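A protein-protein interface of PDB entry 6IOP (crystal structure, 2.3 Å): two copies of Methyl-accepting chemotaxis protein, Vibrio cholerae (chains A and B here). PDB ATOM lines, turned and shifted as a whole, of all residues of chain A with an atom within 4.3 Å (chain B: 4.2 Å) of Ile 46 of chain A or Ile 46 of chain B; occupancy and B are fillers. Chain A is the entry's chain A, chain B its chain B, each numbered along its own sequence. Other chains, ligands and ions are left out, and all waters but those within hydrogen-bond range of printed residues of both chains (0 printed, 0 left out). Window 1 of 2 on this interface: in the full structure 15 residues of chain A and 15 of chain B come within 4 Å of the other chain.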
ATOM      1  N   SER A  42     -30.332  26.940  19.397  1.00  0.00           N
ATOM      2  CA  SER A  42     -29.053  26.372  19.822  1.00  0.00           C
ATOM      3  C   SER A  42     -28.009  26.336  18.711  1.00  0.00           C
ATOM      4  O   SER A  42     -26.841  26.600  18.951  1.00  0.00           O
ATOM      5  CB  SER A  42     -29.242  24.946  20.372  1.00  0.00           C
ATOM      6  OG  SER A  42     -29.550  24.983  21.751  1.00  0.00           O
ATOM      7  N   THR A  43     -28.429  25.979  17.506  1.00  0.00           N
ATOM      8  CA  THR A  43     -27.528  25.972  16.364  1.00  0.00           C
ATOM      9  C   THR A  43     -27.015  27.379  16.055  1.00  0.00           C
ATOM     10  O   THR A  43     -25.878  27.563  15.636  1.00  0.00           O
ATOM     11  CB  THR A  43     -28.222  25.408  15.127  1.00  0.00           C
ATOM     12  OG1 THR A  43     -28.601  24.051  15.387  1.00  0.00           O
ATOM     13  CG2 THR A  43     -27.300  25.464  13.917  1.00  0.00           C
ATOM     14  N   THR A  44     -27.870  28.369  16.275  1.00  0.00           N
ATOM     15  CA  THR A  44     -27.510  29.747  15.986  1.00  0.00           C
ATOM     16  C   THR A  44     -26.485  30.207  17.019  1.00  0.00           C
ATOM     17  O   THR A  44     -25.459  30.792  16.674  1.00  0.00           O
ATOM     18  CB  THR A  44     -28.758  30.668  15.990  1.00  0.00           C
ATOM     19  OG1 THR A  44     -29.721  30.175  15.045  1.00  0.00           O
ATOM     20  CG2 THR A  44     -28.376  32.078  15.634  1.00  0.00           C
ATOM     21  N   GLU A  45     -26.756  29.902  18.285  1.00  0.00           N
ATOM     22  CA  GLU A  45     -25.862  30.296  19.362  1.00  0.00           C
ATOM     23  C   GLU A  45     -24.485  29.666  19.203  1.00  0.00           C
ATOM     24  O   GLU A  45     -23.470  30.292  19.473  1.00  0.00           O
ATOM     25  CB  GLU A  45     -26.474  29.938  20.712  1.00  0.00           C
ATOM     26  CG  GLU A  45     -27.632  30.851  21.047  1.00  0.00           C
ATOM     27  CD  GLU A  45     -28.381  30.457  22.308  1.00  0.00           C
ATOM     28  OE1 GLU A  45     -27.964  29.497  22.994  1.00  0.00           O
ATOM     29  OE2 GLU A  45     -29.399  31.117  22.613  1.00  0.00           O
ATOM     30  N   ILE A  46     -24.465  28.422  18.760  1.00  0.00           N
ATOM     31  CA  ILE A  46     -23.227  27.719  18.534  1.00  0.00           C
ATOM     32  C   ILE A  46     -22.454  28.358  17.367  1.00  0.00           C
ATOM     33  O   ILE A  46     -21.226  28.477  17.414  1.00  0.00           O
ATOM     34  CB  ILE A  46     -23.512  26.213  18.285  1.00  0.00           C
ATOM     35  CG1 ILE A  46     -23.609  25.479  19.632  1.00  0.00           C
ATOM     36  CG2 ILE A  46     -22.463  25.566  17.348  1.00  0.00           C
ATOM     37  CD1 ILE A  46     -24.355  24.163  19.578  1.00  0.00           C
ATOM     38  N   LEU A  47     -23.160  28.792  16.328  1.00  0.00           N
ATOM     39  CA  LEU A  47     -22.447  29.351  15.190  1.00  0.00           C
ATOM     40  C   LEU A  47     -21.865  30.707  15.545  1.00  0.00           C
ATOM     41  O   LEU A  47     -20.851  31.088  14.982  1.00  0.00           O
ATOM     42  CB  LEU A  47     -23.334  29.465  13.947  1.00  0.00           C
ATOM     43  CG  LEU A  47     -23.432  28.154  13.159  1.00  0.00           C
ATOM     44  CD1 LEU A  47     -24.033  28.379  11.789  1.00  0.00           C
ATOM     45  CD2 LEU A  47     -22.054  27.469  13.036  1.00  0.00           C
ATOM     46  N   GLN A  48     -22.454  31.420  16.502  1.00  0.00           N
ATOM     47  CA  GLN A  48     -21.865  32.696  16.863  1.00  0.00           C
ATOM     48  C   GLN A  48     -20.728  32.528  17.881  1.00  0.00           C
ATOM     49  O   GLN A  48     -20.269  33.504  18.475  1.00  0.00           O
ATOM     50  CB  GLN A  48     -22.933  33.708  17.332  1.00  0.00           C
ATOM     51  CG  GLN A  48     -23.751  33.416  18.543  1.00  0.00           C
ATOM     52  CD  GLN A  48     -24.885  34.436  18.727  1.00  0.00           C
ATOM     53  OE1 GLN A  48     -25.387  35.029  17.764  1.00  0.00           O
ATOM     54  NE2 GLN A  48     -25.297  34.632  19.968  1.00  0.00           N
ATOM     55  N   LEU A  49     -20.234  31.298  18.031  1.00  0.00           N
ATOM     56  CA  LEU A  49     -18.905  31.093  18.618  1.00  0.00           C
ATOM     57  C   LEU A  49     -17.818  31.540  17.616  1.00  0.00           C
ATOM     58  O   LEU A  49     -16.772  32.043  18.024  1.00  0.00           O
ATOM     59  CB  LEU A  49     -18.669  29.629  19.021  1.00  0.00           C
ATOM     60  CG  LEU A  49     -19.494  28.991  20.144  1.00  0.00           C
ATOM     61  CD1 LEU A  49     -19.063  27.534  20.353  1.00  0.00           C
ATOM     62  CD2 LEU A  49     -19.424  29.771  21.435  1.00  0.00           C
ATOM     63  N   PHE A  56     -16.491  26.275   9.509  1.00  0.00           N
ATOM     64  CA  PHE A  56     -17.150  25.875  10.743  1.00  0.00           C
ATOM     65  C   PHE A  56     -18.660  25.770  10.531  1.00  0.00           C
ATOM     66  O   PHE A  56     -19.281  24.763  10.861  1.00  0.00           O
ATOM     67  CB  PHE A  56     -16.826  26.889  11.848  1.00  0.00           C
ATOM     68  CG  PHE A  56     -17.547  26.641  13.163  1.00  0.00           C
ATOM     69  CD1 PHE A  56     -17.441  25.423  13.819  1.00  0.00           C
ATOM     70  CD2 PHE A  56     -18.297  27.648  13.757  1.00  0.00           C
ATOM     71  CE1 PHE A  56     -18.083  25.209  15.029  1.00  0.00           C
ATOM     72  CE2 PHE A  56     -18.938  27.444  14.965  1.00  0.00           C
ATOM     73  CZ  PHE A  56     -18.834  26.224  15.602  1.00  0.00           C
ATOM     74  N   VAL A  60     -21.153  22.386  10.593  1.00  0.00           N
ATOM     75  CA  VAL A  60     -22.282  22.285  11.493  1.00  0.00           C
ATOM     76  C   VAL A  60     -23.547  21.948  10.706  1.00  0.00           C
ATOM     77  O   VAL A  60     -24.206  20.957  11.001  1.00  0.00           O
ATOM     78  CB  VAL A  60     -22.461  23.576  12.302  1.00  0.00           C
ATOM     79  CG1 VAL A  60     -23.802  23.574  13.062  1.00  0.00           C
ATOM     80  CG2 VAL A  60     -21.269  23.741  13.252  1.00  0.00           C
ATOM     81  N   SER B  42     -27.794  16.375  18.178  1.00  0.00           N
ATOM     82  CA  SER B  42     -27.118  17.365  17.340  1.00  0.00           C
ATOM     83  C   SER B  42     -25.905  17.948  18.041  1.00  0.00           C
ATOM     84  O   SER B  42     -24.846  18.076  17.446  1.00  0.00           O
ATOM     85  CB  SER B  42     -28.074  18.487  16.939  1.00  0.00           C
ATOM     86  OG  SER B  42     -28.749  18.169  15.733  1.00  0.00           O
ATOM     87  N   THR B  43     -26.077  18.285  19.311  1.00  0.00           N
ATOM     88  CA  THR B  43     -25.002  18.779  20.128  1.00  0.00           C
ATOM     89  C   THR B  43     -23.821  17.806  20.122  1.00  0.00           C
ATOM     90  O   THR B  43     -22.663  18.217  20.042  1.00  0.00           O
ATOM     91  CB  THR B  43     -25.463  18.989  21.569  1.00  0.00           C
ATOM     92  OG1 THR B  43     -26.656  19.790  21.585  1.00  0.00           O
ATOM     93  CG2 THR B  43     -24.353  19.652  22.388  1.00  0.00           C
ATOM     94  N   THR B  44     -24.138  16.516  20.226  1.00  0.00           N
ATOM     95  CA  THR B  44     -23.138  15.463  20.173  1.00  0.00           C
ATOM     96  C   THR B  44     -22.442  15.407  18.814  1.00  0.00           C
ATOM     97  O   THR B  44     -21.233  15.263  18.750  1.00  0.00           O
ATOM     98  CB  THR B  44     -23.754  14.083  20.486  1.00  0.00           C
ATOM     99  OG1 THR B  44     -24.280  14.081  21.818  1.00  0.00           O
ATOM    100  CG2 THR B  44     -22.703  12.988  20.371  1.00  0.00           C
ATOM    101  N   GLU B  45     -23.199  15.520  17.729  1.00  0.00           N
ATOM    102  CA  GLU B  45     -22.587  15.510  16.412  1.00  0.00           C
ATOM    103  C   GLU B  45     -21.729  16.756  16.184  1.00  0.00           C
ATOM    104  O   GLU B  45     -20.718  16.691  15.500  1.00  0.00           O
ATOM    105  CB  GLU B  45     -23.648  15.385  15.335  1.00  0.00           C
ATOM    106  CG  GLU B  45     -24.294  14.014  15.318  1.00  0.00           C
ATOM    107  CD  GLU B  45     -25.511  13.956  14.414  1.00  0.00           C
ATOM    108  OE1 GLU B  45     -25.869  15.002  13.818  1.00  0.00           O
ATOM    109  OE2 GLU B  45     -26.109  12.865  14.293  1.00  0.00           O
ATOM    110  N   ILE B  46     -22.110  17.881  16.779  1.00  0.00           N
ATOM    111  CA  ILE B  46     -21.311  19.088  16.634  1.00  0.00           C
ATOM    112  C   ILE B  46     -19.987  18.952  17.400  1.00  0.00           C
ATOM    113  O   ILE B  46     -18.931  19.280  16.872  1.00  0.00           O
ATOM    114  CB  ILE B  46     -22.086  20.334  17.096  1.00  0.00           C
ATOM    115  CG1 ILE B  46     -23.261  20.578  16.149  1.00  0.00           C
ATOM    116  CG2 ILE B  46     -21.179  21.567  17.086  1.00  0.00           C
ATOM    117  CD1 ILE B  46     -24.093  21.768  16.514  1.00  0.00           C
ATOM    118  N   LEU B  47     -20.037  18.445  18.627  1.00  0.00           N
ATOM    119  CA  LEU B  47     -18.810  18.192  19.377  1.00  0.00           C
ATOM    120  C   LEU B  47     -17.908  17.155  18.693  1.00  0.00           C
ATOM    121  O   LEU B  47     -16.698  17.115  18.935  1.00  0.00           O
ATOM    122  CB  LEU B  47     -19.127  17.745  20.794  1.00  0.00           C
ATOM    123  CG  LEU B  47     -19.671  18.846  21.693  1.00  0.00           C
ATOM    124  CD1 LEU B  47     -19.594  18.412  23.138  1.00  0.00           C
ATOM    125  CD2 LEU B  47     -18.922  20.154  21.464  1.00  0.00           C
ATOM    126  N   GLN B  48     -18.482  16.341  17.813  1.00  0.00           N
ATOM    127  CA  GLN B  48     -17.684  15.358  17.097  1.00  0.00           C
ATOM    128  C   GLN B  48     -16.910  15.981  15.933  1.00  0.00           C
ATOM    129  O   GLN B  48     -16.272  15.276  15.155  1.00  0.00           O
ATOM    130  CB  GLN B  48     -18.569  14.214  16.608  1.00  0.00           C
ATOM    131  CG  GLN B  48     -18.821  13.205  17.703  1.00  0.00           C
ATOM    132  CD  GLN B  48     -19.564  11.980  17.233  1.00  0.00           C
ATOM    133  OE1 GLN B  48     -19.575  10.960  17.913  1.00  0.00           O
ATOM    134  NE2 GLN B  48     -20.196  12.073  16.072  1.00  0.00           N
ATOM    135  N   LEU B  49     -16.974  17.304  15.823  1.00  0.00           N
ATOM    136  CA  LEU B  49     -16.198  18.034  14.835  1.00  0.00           C
ATOM    137  C   LEU B  49     -14.803  18.292  15.415  1.00  0.00           C
ATOM    138  O   LEU B  49     -13.841  18.442  14.671  1.00  0.00           O
ATOM    139  CB  LEU B  49     -16.892  19.350  14.438  1.00  0.00           C
ATOM    140  CG  LEU B  49     -18.244  19.240  13.700  1.00  0.00           C
ATOM    141  CD1 LEU B  49     -18.909  20.601  13.476  1.00  0.00           C
ATOM    142  CD2 LEU B  49     -18.121  18.497  12.368  1.00  0.00           C
ATOM    143  N   PHE B  56     -13.602  23.962  23.309  1.00  0.00           N
ATOM    144  CA  PHE B  56     -14.695  24.019  22.359  1.00  0.00           C
ATOM    145  C   PHE B  56     -15.978  23.428  22.966  1.00  0.00           C
ATOM    146  O   PHE B  56     -17.011  24.103  23.075  1.00  0.00           O
ATOM    147  CB  PHE B  56     -14.308  23.262  21.092  1.00  0.00           C
ATOM    148  CG  PHE B  56     -15.426  23.118  20.110  1.00  0.00           C
ATOM    149  CD1 PHE B  56     -16.067  24.237  19.601  1.00  0.00           C
ATOM    150  CD2 PHE B  56     -15.840  21.866  19.686  1.00  0.00           C
ATOM    151  CE1 PHE B  56     -17.117  24.104  18.685  1.00  0.00           C
ATOM    152  CE2 PHE B  56     -16.882  21.733  18.772  1.00  0.00           C
ATOM    153  CZ  PHE B  56     -17.522  22.859  18.277  1.00  0.00           C
ATOM    154  N   VAL B  60     -19.597  25.274  23.741  1.00  0.00           N
ATOM    155  CA  VAL B  60     -20.865  24.787  23.235  1.00  0.00           C
ATOM    156  C   VAL B  60     -21.837  24.541  24.382  1.00  0.00           C
ATOM    157  O   VAL B  60     -22.981  24.988  24.338  1.00  0.00           O
ATOM    158  CB  VAL B  60     -20.671  23.520  22.427  1.00  0.00           C
ATOM    159  CG1 VAL B  60     -22.025  22.930  22.024  1.00  0.00           C
ATOM    160  CG2 VAL B  60     -19.818  23.824  21.184  1.00  0.00           C
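Hydrophobic or aromatic side chains of chain A within 4 Å of the printed part of chain B: Ile 46, Leu 49, Phe 56 and Val 60.
Among the printed residues, 6 pairs touch across the chains.
Among the printed residues, no Asp or Glu carboxylate lies within 4 Å of a Lys or Arg side-chain nitrogen of the other chain.
Of chain B, only Ile 46 (3.9 Å) and Val 60 (3.6 Å) come within 4 Å of Ile 46 of chain A.
Printed residues of chain A within 4 Å of Leu 49 of chain B: Val 60 (3.9 Å).
Of the printed residues of chain B, Phe 56 of chain A touches Phe 56 (3.9 Å).
Thr 44 of chain A touches none of the printed residues of chain B.
The nearest printed residue of chain A that does not touch Ile 46 of chain B is Thr 43 of chain A (5.2 Å).
The nearest printed residue of chain B that does not touch Leu 49 of chain A is Phe 56 of chain B (4.3 Å).
Ile 46 of chain A touches its own counterpart, Ile 46 of chain B.
Ile 46 of chain A touches Val 60 of chain B, and with the chains exchanged Val 60 of chain A touches Ile 46 of chain B.
Leu 49 of chain A touches Val 60 of chain B, and with the chains exchanged Val 60 of chain A touches Leu 49 of chain B.
Phe 56 of chain B touches its own counterpart, Phe 56 of chain A.
Positions printed for both chains: 42, 43, 44, 45, 46, 47, 48, 49, 56 and 60.
Of the 6 pairs that touch across the chains among the printed residues, 6 have their exchanged pair printed and touching as well.
Ile 46 of chain B touches Ile 46 of chain A.
CG1 of Val 60 of chain B touches CD1 of Ile 46 of chain A, 3.6 Å away.
Val 60 of chain B touches Leu 49 of chain A (CG2 to CD1, 3.9 Å).
Phe 56 of chain B touches Phe 56 of chain A.
CD1 of Ile 46 of chain B touches CG1 of Val 60 of chain A (3.9 Å).
Leu 49 of chain B touches Val 60 of chain A.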
